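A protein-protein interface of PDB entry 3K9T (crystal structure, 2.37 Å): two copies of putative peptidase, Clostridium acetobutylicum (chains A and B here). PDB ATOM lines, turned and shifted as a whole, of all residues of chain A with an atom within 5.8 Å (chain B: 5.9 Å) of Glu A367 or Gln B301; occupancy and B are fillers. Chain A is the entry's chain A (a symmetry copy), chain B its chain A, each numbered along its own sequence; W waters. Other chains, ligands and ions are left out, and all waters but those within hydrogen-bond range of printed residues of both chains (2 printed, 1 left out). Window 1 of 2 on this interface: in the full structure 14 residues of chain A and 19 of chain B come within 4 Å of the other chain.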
ATOM      1  N   ASN A 363      -6.706   2.350   7.734  1.00  0.00           N
ATOM      2  CA  ASN A 363      -7.216   1.656   6.546  1.00  0.00           C
ATOM      3  C   ASN A 363      -6.211   1.851   5.401  1.00  0.00           C
ATOM      4  O   ASN A 363      -6.510   2.457   4.384  1.00  0.00           O
ATOM      5  CB  ASN A 363      -8.587   2.213   6.141  1.00  0.00           C
ATOM      6  CG  ASN A 363      -9.272   1.372   5.064  1.00  0.00           C
ATOM      7  OD1 ASN A 363      -9.949   0.404   5.373  1.00  0.00           O
ATOM      8  ND2 ASN A 363      -9.103   1.755   3.799  1.00  0.00           N
ATOM      9  N   PRO A 364      -5.007   1.331   5.558  1.00  0.00           N
ATOM     10  CA  PRO A 364      -3.982   1.613   4.548  1.00  0.00           C
ATOM     11  C   PRO A 364      -4.162   0.875   3.218  1.00  0.00           C
ATOM     12  O   PRO A 364      -3.617   1.320   2.216  1.00  0.00           O
ATOM     13  CB  PRO A 364      -2.699   1.157   5.234  1.00  0.00           C
ATOM     14  CG  PRO A 364      -3.155   0.003   6.138  1.00  0.00           C
ATOM     15  CD  PRO A 364      -4.548   0.391   6.595  1.00  0.00           C
ATOM     16  N   LYS A 365      -4.890  -0.243   3.219  1.00  0.00           N
ATOM     17  CA  LYS A 365      -5.123  -1.017   2.009  1.00  0.00           C
ATOM     18  C   LYS A 365      -6.226  -0.398   1.140  1.00  0.00           C
ATOM     19  O   LYS A 365      -7.408  -0.626   1.342  1.00  0.00           O
ATOM     20  CB  LYS A 365      -5.423  -2.485   2.317  1.00  0.00           C
ATOM     21  CG  LYS A 365      -4.238  -3.211   2.913  1.00  0.00           C
ATOM     22  CD  LYS A 365      -4.500  -4.709   2.974  1.00  0.00           C
ATOM     23  CE  LYS A 365      -3.599  -5.427   3.998  1.00  0.00           C
ATOM     24  NZ  LYS A 365      -4.080  -6.829   4.250  1.00  0.00           N
ATOM     25  N   CYS A 366      -5.784   0.369   0.146  1.00  0.00           N
ATOM     26  CA  CYS A 366      -6.639   1.174  -0.697  1.00  0.00           C
ATOM     27  C   CYS A 366      -7.333   2.250   0.106  1.00  0.00           C
ATOM     28  O   CYS A 366      -7.307   2.287   1.356  1.00  0.00           O
ATOM     29  CB  CYS A 366      -7.635   0.330  -1.445  1.00  0.00           C
ATOM     30  SG  CYS A 366      -6.853  -0.932  -2.394  1.00  0.00           S
ATOM     31  N   GLU A 367      -7.950   3.163  -0.612  1.00  0.00           N
ATOM     32  CA  GLU A 367      -8.603   4.252   0.086  1.00  0.00           C
ATOM     33  C   GLU A 367      -9.870   3.729   0.739  1.00  0.00           C
ATOM     34  O   GLU A 367     -10.397   2.675   0.356  1.00  0.00           O
ATOM     35  CB  GLU A 367      -8.768   5.523  -0.787  1.00  0.00           C
ATOM     36  CG  GLU A 367      -9.492   5.427  -2.089  1.00  0.00           C
ATOM     37  CD  GLU A 367      -9.274   6.645  -3.002  1.00  0.00           C
ATOM     38  OE1 GLU A 367      -8.227   7.329  -2.962  1.00  0.00           O
ATOM     39  OE2 GLU A 367     -10.177   6.895  -3.810  1.00  0.00           O
ATOM     40  N   PRO A 368     -10.296   4.385   1.814  1.00  0.00           N
ATOM     41  CA  PRO A 368     -11.533   3.979   2.446  1.00  0.00           C
ATOM     42  C   PRO A 368     -12.681   4.430   1.586  1.00  0.00           C
ATOM     43  O   PRO A 368     -12.523   5.371   0.806  1.00  0.00           O
ATOM     44  CB  PRO A 368     -11.529   4.756   3.762  1.00  0.00           C
ATOM     45  CG  PRO A 368     -10.655   5.894   3.542  1.00  0.00           C
ATOM     46  CD  PRO A 368      -9.629   5.473   2.539  1.00  0.00           C
ATOM     47  N   GLN A 369     -13.822   3.773   1.716  1.00  0.00           N
ATOM     48  CA  GLN A 369     -14.999   4.198   0.980  1.00  0.00           C
ATOM     49  C   GLN A 369     -15.567   5.399   1.746  1.00  0.00           C
ATOM     50  O   GLN A 369     -16.468   5.233   2.561  1.00  0.00           O
ATOM     51  CB  GLN A 369     -15.979   3.030   0.884  1.00  0.00           C
ATOM     52  CG  GLN A 369     -17.216   3.288   0.048  1.00  0.00           C
ATOM     53  CD  GLN A 369     -17.931   2.022  -0.354  1.00  0.00           C
ATOM     54  OE1 GLN A 369     -17.773   0.964   0.271  1.00  0.00           O
ATOM     55  NE2 GLN A 369     -18.721   2.115  -1.420  1.00  0.00           N
ATOM     56  N   PHE A 393      -6.899  13.082   1.218  1.00  0.00           N
ATOM     57  CA  PHE A 393      -6.251  12.021   0.444  1.00  0.00           C
ATOM     58  C   PHE A 393      -4.738  11.989   0.644  1.00  0.00           C
ATOM     59  O   PHE A 393      -4.143  10.911   0.657  1.00  0.00           O
ATOM     60  CB  PHE A 393      -6.570  12.130  -1.044  1.00  0.00           C
ATOM     61  CG  PHE A 393      -7.987  11.768  -1.398  1.00  0.00           C
ATOM     62  CD1 PHE A 393      -8.526  10.544  -1.019  1.00  0.00           C
ATOM     63  CD2 PHE A 393      -8.760  12.626  -2.188  1.00  0.00           C
ATOM     64  CE1 PHE A 393      -9.829  10.202  -1.375  1.00  0.00           C
ATOM     65  CE2 PHE A 393     -10.063  12.300  -2.533  1.00  0.00           C
ATOM     66  CZ  PHE A 393     -10.592  11.075  -2.137  1.00  0.00           C
ATOM     67  N   LEU A 396      -4.151  10.507   4.241  1.00  0.00           N
ATOM     68  CA  LEU A 396      -4.334   9.055   4.226  1.00  0.00           C
ATOM     69  C   LEU A 396      -3.179   8.384   3.519  1.00  0.00           C
ATOM     70  O   LEU A 396      -2.675   7.347   3.963  1.00  0.00           O
ATOM     71  CB  LEU A 396      -5.649   8.668   3.544  1.00  0.00           C
ATOM     72  CG  LEU A 396      -6.912   9.043   4.341  1.00  0.00           C
ATOM     73  CD1 LEU A 396      -8.137   9.084   3.465  1.00  0.00           C
ATOM     74  CD2 LEU A 396      -7.095   8.032   5.470  1.00  0.00           C
ATOM     75  N   ASP B  64     -12.219  -1.984   2.386  1.00  0.00           N
ATOM     76  CA  ASP B  64     -13.221  -1.131   3.032  1.00  0.00           C
ATOM     77  C   ASP B  64     -14.441  -0.930   2.174  1.00  0.00           C
ATOM     78  O   ASP B  64     -15.440  -0.399   2.635  1.00  0.00           O
ATOM     79  CB  ASP B  64     -12.647   0.258   3.378  1.00  0.00           C
ATOM     80  CG  ASP B  64     -13.500   1.003   4.375  1.00  0.00           C
ATOM     81  OD1 ASP B  64     -13.890   0.385   5.389  1.00  0.00           O
ATOM     82  OD2 ASP B  64     -13.799   2.198   4.143  1.00  0.00           O
ATOM     83  N   TRP B  65     -14.371  -1.364   0.924  1.00  0.00           N
ATOM     84  CA  TRP B  65     -15.482  -1.139   0.008  1.00  0.00           C
ATOM     85  C   TRP B  65     -16.402  -2.335  -0.096  1.00  0.00           C
ATOM     86  O   TRP B  65     -16.050  -3.440   0.284  1.00  0.00           O
ATOM     87  CB  TRP B  65     -14.955  -0.761  -1.378  1.00  0.00           C
ATOM     88  CG  TRP B  65     -14.272   0.535  -1.411  1.00  0.00           C
ATOM     89  CD1 TRP B  65     -13.136   0.886  -0.737  1.00  0.00           C
ATOM     90  CD2 TRP B  65     -14.663   1.687  -2.174  1.00  0.00           C
ATOM     91  NE1 TRP B  65     -12.792   2.185  -1.042  1.00  0.00           N
ATOM     92  CE2 TRP B  65     -13.710   2.696  -1.923  1.00  0.00           C
ATOM     93  CE3 TRP B  65     -15.703   1.948  -3.067  1.00  0.00           C
ATOM     94  CZ2 TRP B  65     -13.776   3.944  -2.518  1.00  0.00           C
ATOM     95  CZ3 TRP B  65     -15.777   3.213  -3.662  1.00  0.00           C
ATOM     96  CH2 TRP B  65     -14.817   4.186  -3.378  1.00  0.00           C
ATOM     97  N   THR B 228     -11.482   2.700  -9.607  1.00  0.00           N
ATOM     98  CA  THR B 228     -11.602   2.697  -8.175  1.00  0.00           C
ATOM     99  C   THR B 228     -12.127   1.378  -7.655  1.00  0.00           C
ATOM    100  O   THR B 228     -11.353   0.609  -7.138  1.00  0.00           O
ATOM    101  CB  THR B 228     -12.376   3.959  -7.626  1.00  0.00           C
ATOM    102  OG1 THR B 228     -11.601   5.094  -7.959  1.00  0.00           O
ATOM    103  CG2 THR B 228     -12.530   3.961  -6.097  1.00  0.00           C
ATOM    104  N   SER B 231     -10.187  -1.720  -9.338  1.00  0.00           N
ATOM    105  CA  SER B 231      -8.820  -1.917  -8.817  1.00  0.00           C
ATOM    106  C   SER B 231      -8.802  -2.387  -7.364  1.00  0.00           C
ATOM    107  O   SER B 231      -7.998  -3.256  -6.997  1.00  0.00           O
ATOM    108  CB  SER B 231      -7.959  -0.666  -9.004  1.00  0.00           C
ATOM    109  OG  SER B 231      -8.467   0.458  -8.324  1.00  0.00           O
ATOM    110  N   ILE B 232      -9.697  -1.840  -6.542  1.00  0.00           N
ATOM    111  CA  ILE B 232      -9.820  -2.284  -5.130  1.00  0.00           C
ATOM    112  C   ILE B 232     -10.246  -3.758  -5.107  1.00  0.00           C
ATOM    113  O   ILE B 232      -9.634  -4.565  -4.428  1.00  0.00           O
ATOM    114  CB  ILE B 232     -10.804  -1.400  -4.313  1.00  0.00           C
ATOM    115  CG1 ILE B 232     -10.297   0.052  -4.262  1.00  0.00           C
ATOM    116  CG2 ILE B 232     -10.956  -1.939  -2.865  1.00  0.00           C
ATOM    117  CD1 ILE B 232     -11.287   1.049  -3.650  1.00  0.00           C
ATOM    118  N   LEU B 235      -7.222  -5.905  -6.228  1.00  0.00           N
ATOM    119  CA  LEU B 235      -6.209  -5.964  -5.161  1.00  0.00           C
ATOM    120  C   LEU B 235      -6.698  -6.882  -4.023  1.00  0.00           C
ATOM    121  O   LEU B 235      -5.923  -7.660  -3.469  1.00  0.00           O
ATOM    122  CB  LEU B 235      -5.842  -4.554  -4.647  1.00  0.00           C
ATOM    123  CG  LEU B 235      -4.983  -3.716  -5.589  1.00  0.00           C
ATOM    124  CD1 LEU B 235      -4.887  -2.242  -5.194  1.00  0.00           C
ATOM    125  CD2 LEU B 235      -3.594  -4.337  -5.695  1.00  0.00           C
ATOM    126  N   PRO B 294      -2.281  11.864  -4.758  1.00  0.00           N
ATOM    127  CA  PRO B 294      -3.215  10.780  -4.450  1.00  0.00           C
ATOM    128  C   PRO B 294      -4.695  11.034  -4.894  1.00  0.00           C
ATOM    129  O   PRO B 294      -5.658  10.795  -4.152  1.00  0.00           O
ATOM    130  CB  PRO B 294      -3.075  10.646  -2.940  1.00  0.00           C
ATOM    131  CG  PRO B 294      -2.939  12.081  -2.512  1.00  0.00           C
ATOM    132  CD  PRO B 294      -2.129  12.757  -3.605  1.00  0.00           C
ATOM    133  N   SER B 297      -6.558   8.756 -11.246  1.00  0.00           N
ATOM    134  CA  SER B 297      -7.025   7.402 -11.550  1.00  0.00           C
ATOM    135  C   SER B 297      -6.452   6.367 -10.581  1.00  0.00           C
ATOM    136  O   SER B 297      -6.039   6.729  -9.503  1.00  0.00           O
ATOM    137  CB  SER B 297      -6.767   7.025 -13.006  1.00  0.00           C
ATOM    138  OG  SER B 297      -7.543   5.883 -13.342  1.00  0.00           O
ATOM    139  N   ASP B 298      -6.424   5.089 -10.976  1.00  0.00           N
ATOM    140  CA  ASP B 298      -6.187   3.962 -10.023  1.00  0.00           C
ATOM    141  C   ASP B 298      -4.818   3.887  -9.372  1.00  0.00           C
ATOM    142  O   ASP B 298      -4.599   3.061  -8.500  1.00  0.00           O
ATOM    143  CB  ASP B 298      -6.535   2.636 -10.666  1.00  0.00           C
ATOM    144  CG  ASP B 298      -8.029   2.509 -10.992  1.00  0.00           C
ATOM    145  OD1 ASP B 298      -8.869   2.683 -10.084  1.00  0.00           O
ATOM    146  OD2 ASP B 298      -8.351   2.220 -12.158  1.00  0.00           O
ATOM    147  N   GLU B 299      -3.894   4.748  -9.787  1.00  0.00           N
ATOM    148  CA  GLU B 299      -2.592   4.860  -9.121  1.00  0.00           C
ATOM    149  C   GLU B 299      -2.775   5.214  -7.647  1.00  0.00           C
ATOM    150  O   GLU B 299      -1.944   4.851  -6.816  1.00  0.00           O
ATOM    151  CB  GLU B 299      -1.687   5.855  -9.840  1.00  0.00           C
ATOM    152  CG  GLU B 299      -2.151   7.303  -9.802  1.00  0.00           C
ATOM    153  CD  GLU B 299      -3.164   7.657 -10.862  1.00  0.00           C
ATOM    154  OE1 GLU B 299      -3.592   6.746 -11.617  1.00  0.00           O
ATOM    155  OE2 GLU B 299      -3.511   8.868 -10.932  1.00  0.00           O
ATOM    156  N   ARG B 300      -3.885   5.879  -7.307  1.00  0.00           N
ATOM    157  CA  ARG B 300      -4.271   6.035  -5.882  1.00  0.00           C
ATOM    158  C   ARG B 300      -4.480   4.751  -5.110  1.00  0.00           C
ATOM    159  O   ARG B 300      -4.116   4.653  -3.929  1.00  0.00           O
ATOM    160  CB  ARG B 300      -5.515   6.899  -5.685  1.00  0.00           C
ATOM    161  CG  ARG B 300      -6.548   6.814  -6.739  1.00  0.00           C
ATOM    162  CD  ARG B 300      -7.306   8.120  -6.812  1.00  0.00           C
ATOM    163  NE  ARG B 300      -8.617   7.897  -6.257  1.00  0.00           N
ATOM    164  CZ  ARG B 300      -9.745   8.006  -6.946  1.00  0.00           C
ATOM    165  NH1 ARG B 300      -9.730   8.437  -8.202  1.00  0.00           N
ATOM    166  NH2 ARG B 300     -10.905   7.721  -6.365  1.00  0.00           N
ATOM    167  N   GLN B 301      -5.095   3.766  -5.737  1.00  0.00           N
ATOM    168  CA  GLN B 301      -5.271   2.493  -5.031  1.00  0.00           C
ATOM    169  C   GLN B 301      -3.926   1.775  -4.979  1.00  0.00           C
ATOM    170  O   GLN B 301      -3.497   1.361  -3.929  1.00  0.00           O
ATOM    171  CB  GLN B 301      -6.384   1.651  -5.638  1.00  0.00           C
ATOM    172  CG  GLN B 301      -7.656   2.440  -5.980  1.00  0.00           C
ATOM    173  CD  GLN B 301      -8.233   3.213  -4.818  1.00  0.00           C
ATOM    174  OE1 GLN B 301      -8.025   2.854  -3.648  1.00  0.00           O
ATOM    175  NE2 GLN B 301      -8.997   4.277  -5.132  1.00  0.00           N
ATOM    176  N   PHE B 302      -3.190   1.738  -6.081  1.00  0.00           N
ATOM    177  CA  PHE B 302      -1.907   1.013  -6.088  1.00  0.00           C
ATOM    178  C   PHE B 302      -0.863   1.657  -5.208  1.00  0.00           C
ATOM    179  O   PHE B 302       0.048   0.987  -4.758  1.00  0.00           O
ATOM    180  CB  PHE B 302      -1.379   0.809  -7.520  1.00  0.00           C
ATOM    181  CG  PHE B 302      -2.301   0.012  -8.375  1.00  0.00           C
ATOM    182  CD1 PHE B 302      -2.605  -1.292  -8.046  1.00  0.00           C
ATOM    183  CD2 PHE B 302      -2.910   0.573  -9.493  1.00  0.00           C
ATOM    184  CE1 PHE B 302      -3.502  -2.037  -8.834  1.00  0.00           C
ATOM    185  CE2 PHE B 302      -3.808  -0.186 -10.290  1.00  0.00           C
ATOM    186  CZ  PHE B 302      -4.093  -1.476  -9.961  1.00  0.00           C
ATOM    187  N   SER B 303      -1.013   2.951  -4.960  1.00  0.00           N
ATOM    188  CA  SER B 303      -0.068   3.718  -4.165  1.00  0.00           C
ATOM    189  C   SER B 303      -0.517   3.968  -2.733  1.00  0.00           C
ATOM    190  O   SER B 303       0.157   4.709  -2.038  1.00  0.00           O
ATOM    191  CB  SER B 303       0.173   5.052  -4.848  1.00  0.00           C
ATOM    192  OG  SER B 303       0.699   4.824  -6.146  1.00  0.00           O
ATOM    193  N   SER B 304      -1.657   3.392  -2.311  1.00  0.00           N
ATOM    194  CA  SER B 304      -2.084   3.385  -0.902  1.00  0.00           C
ATOM    195  C   SER B 304      -0.925   2.853  -0.106  1.00  0.00           C
ATOM    196  O   SER B 304      -0.120   2.074  -0.630  1.00  0.00           O
ATOM    197  CB  SER B 304      -3.185   2.367  -0.600  1.00  0.00           C
ATOM    198  OG  SER B 304      -3.912   1.984  -1.712  1.00  0.00           O
ATOM    199  N   ILE B 307      -0.512  -0.963   0.045  1.00  0.00           N
ATOM    200  CA  ILE B 307      -0.300  -1.670  -1.234  1.00  0.00           C
ATOM    201  C   ILE B 307       1.092  -1.296  -1.702  1.00  0.00           C
ATOM    202  O   ILE B 307       1.945  -2.158  -1.830  1.00  0.00           O
ATOM    203  CB  ILE B 307      -1.394  -1.288  -2.293  1.00  0.00           C
ATOM    204  CG1 ILE B 307      -2.797  -1.624  -1.748  1.00  0.00           C
ATOM    205  CG2 ILE B 307      -1.114  -1.950  -3.626  1.00  0.00           C
ATOM    206  CD1 ILE B 307      -3.049  -3.069  -1.394  1.00  0.00           C
ATOM    207  N   ASN B 308       1.288   0.000  -1.982  1.00  0.00           N
ATOM    208  CA  ASN B 308       2.602   0.612  -2.042  1.00  0.00           C
ATOM    209  C   ASN B 308       3.488   0.106  -3.165  1.00  0.00           C
ATOM    210  O   ASN B 308       4.715  -0.048  -3.005  1.00  0.00           O
ATOM    211  CB  ASN B 308       3.298   0.471  -0.683  1.00  0.00           C
ATOM    212  CG  ASN B 308       4.373   1.519  -0.463  1.00  0.00           C
ATOM    213  OD1 ASN B 308       4.165   2.717  -0.676  1.00  0.00           O
ATOM    214  ND2 ASN B 308       5.529   1.075  -0.031  1.00  0.00           N
HETATM  215  O   HOH W   1     -18.283  -0.819   2.676  1.00  0.00           O
HETATM  216  O   HOH W   2      -5.896   8.468  -2.740  1.00  0.00           O
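N of Gln A369 is in hydrogen-bond range of OD2 of Asp B64, 2.9 Å away.
The indole nitrogen (NE1) of Trp B65 lies within hydrogen-bond range of the backbone carbonyl oxygen (O) of Glu A367 (2.8 Å).
The side-chain carboxylate of Glu A367 is in salt-bridge range of the guanidinium group of Arg B300 (2.8 Å).
The side-chain amide oxygen of Gln B301 lies within hydrogen-bond range of the backbone NH of Glu A367 (3.1 Å).
The side-chain hydroxyl (OG) of Ser B304 lies close to the backbone NH (N) of Cys A366 (3.1 Å).
The backbone NH (N) of Gln A369 lies close to the indole nitrogen (NE1) of Trp B65 (3.3 Å).
NH2 of Arg B300 sits at hydrogen-bond distance from OG1 of Thr B228 (3.2 Å).
The backbone carbonyl oxygen of Arg B300 is in hydrogen-bond range of the side-chain hydroxyl of Ser B304 (3.5 Å).
The side-chain amide nitrogen (ND2) of Asn A363 lies within hydrogen-bond range of the backbone carbonyl oxygen (O) of Cys A366.
Among the printed residues, merely in contact across the chains: Asn A363 with Asp B64 (3.4 Å), Pro A364 with Ser B304 (3.0 Å), Cys A366 with Ile B232 (3.9 Å), Cys A366 with Leu B235 (3.7 Å), Cys A366 with Gln B301 (3.4 Å), Pro A368 with Asp B64 (3.3 Å), Pro A368 with Trp B65 (3.5 Å) and Phe A393 with Pro B294 (3.5 Å).
Printed residues of chain B within 4 Å of Glu A367: Trp B65 (2.8 Å), Arg B300 (2.8 Å) and Gln B301 (3.1 Å).
Printed residues of chain B within 4 Å of Pro A368: Asp B64 (3.3 Å) and Trp B65 (3.5 Å).
Of the printed residues of chain B, Phe A393 touches Pro B294.
Printed residues of chain A within 4 Å of Trp B65: Glu A367, Pro A368 and Gln A369.
Of the printed residues of chain A, Arg B300 touches Glu A367.
Gln B301 touches two residues of chain A.
Printed residues of chain A within 4 Å of Ser B304: Pro A364 (3.0 Å) and Cys A366 (3.0 Å).
The nearest residue of chain B that does not touch Glu A367 is Ser B304 (4.3 Å).
The nearest printed residue of chain A that does not touch Gln B301 is Lys A365 (6.0 Å).
Along chain B the printed residues that touch a printed residue of chain A span positions 64 to 304.
Of the 9 printed residues of chain A, 7 touch a printed residue of chain B.
Hydrophobic or aromatic side chains of chain A within 4 Å of the printed part of chain B: Pro A368 and Phe A393.
Along chain A the printed residues that touch a printed residue of chain B span positions 363 to 393.
Among the printed residues, 14 pairs touch across the chains.
Among the printed residues, Asp or Glu carboxylates within 4 Å of a Lys or Arg side-chain nitrogen of the other chain: Glu A367 with Arg B300.
No position is printed for both chains.
Water W2 lies within hydrogen-bond range of OE1 of Glu A367 and O of Pro B294.
Water W1 bridges the backbone carbonyl oxygen of Asp B64 (2.9 Å) and the side-chain amide oxygen of Gln A369 (3.0 Å).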
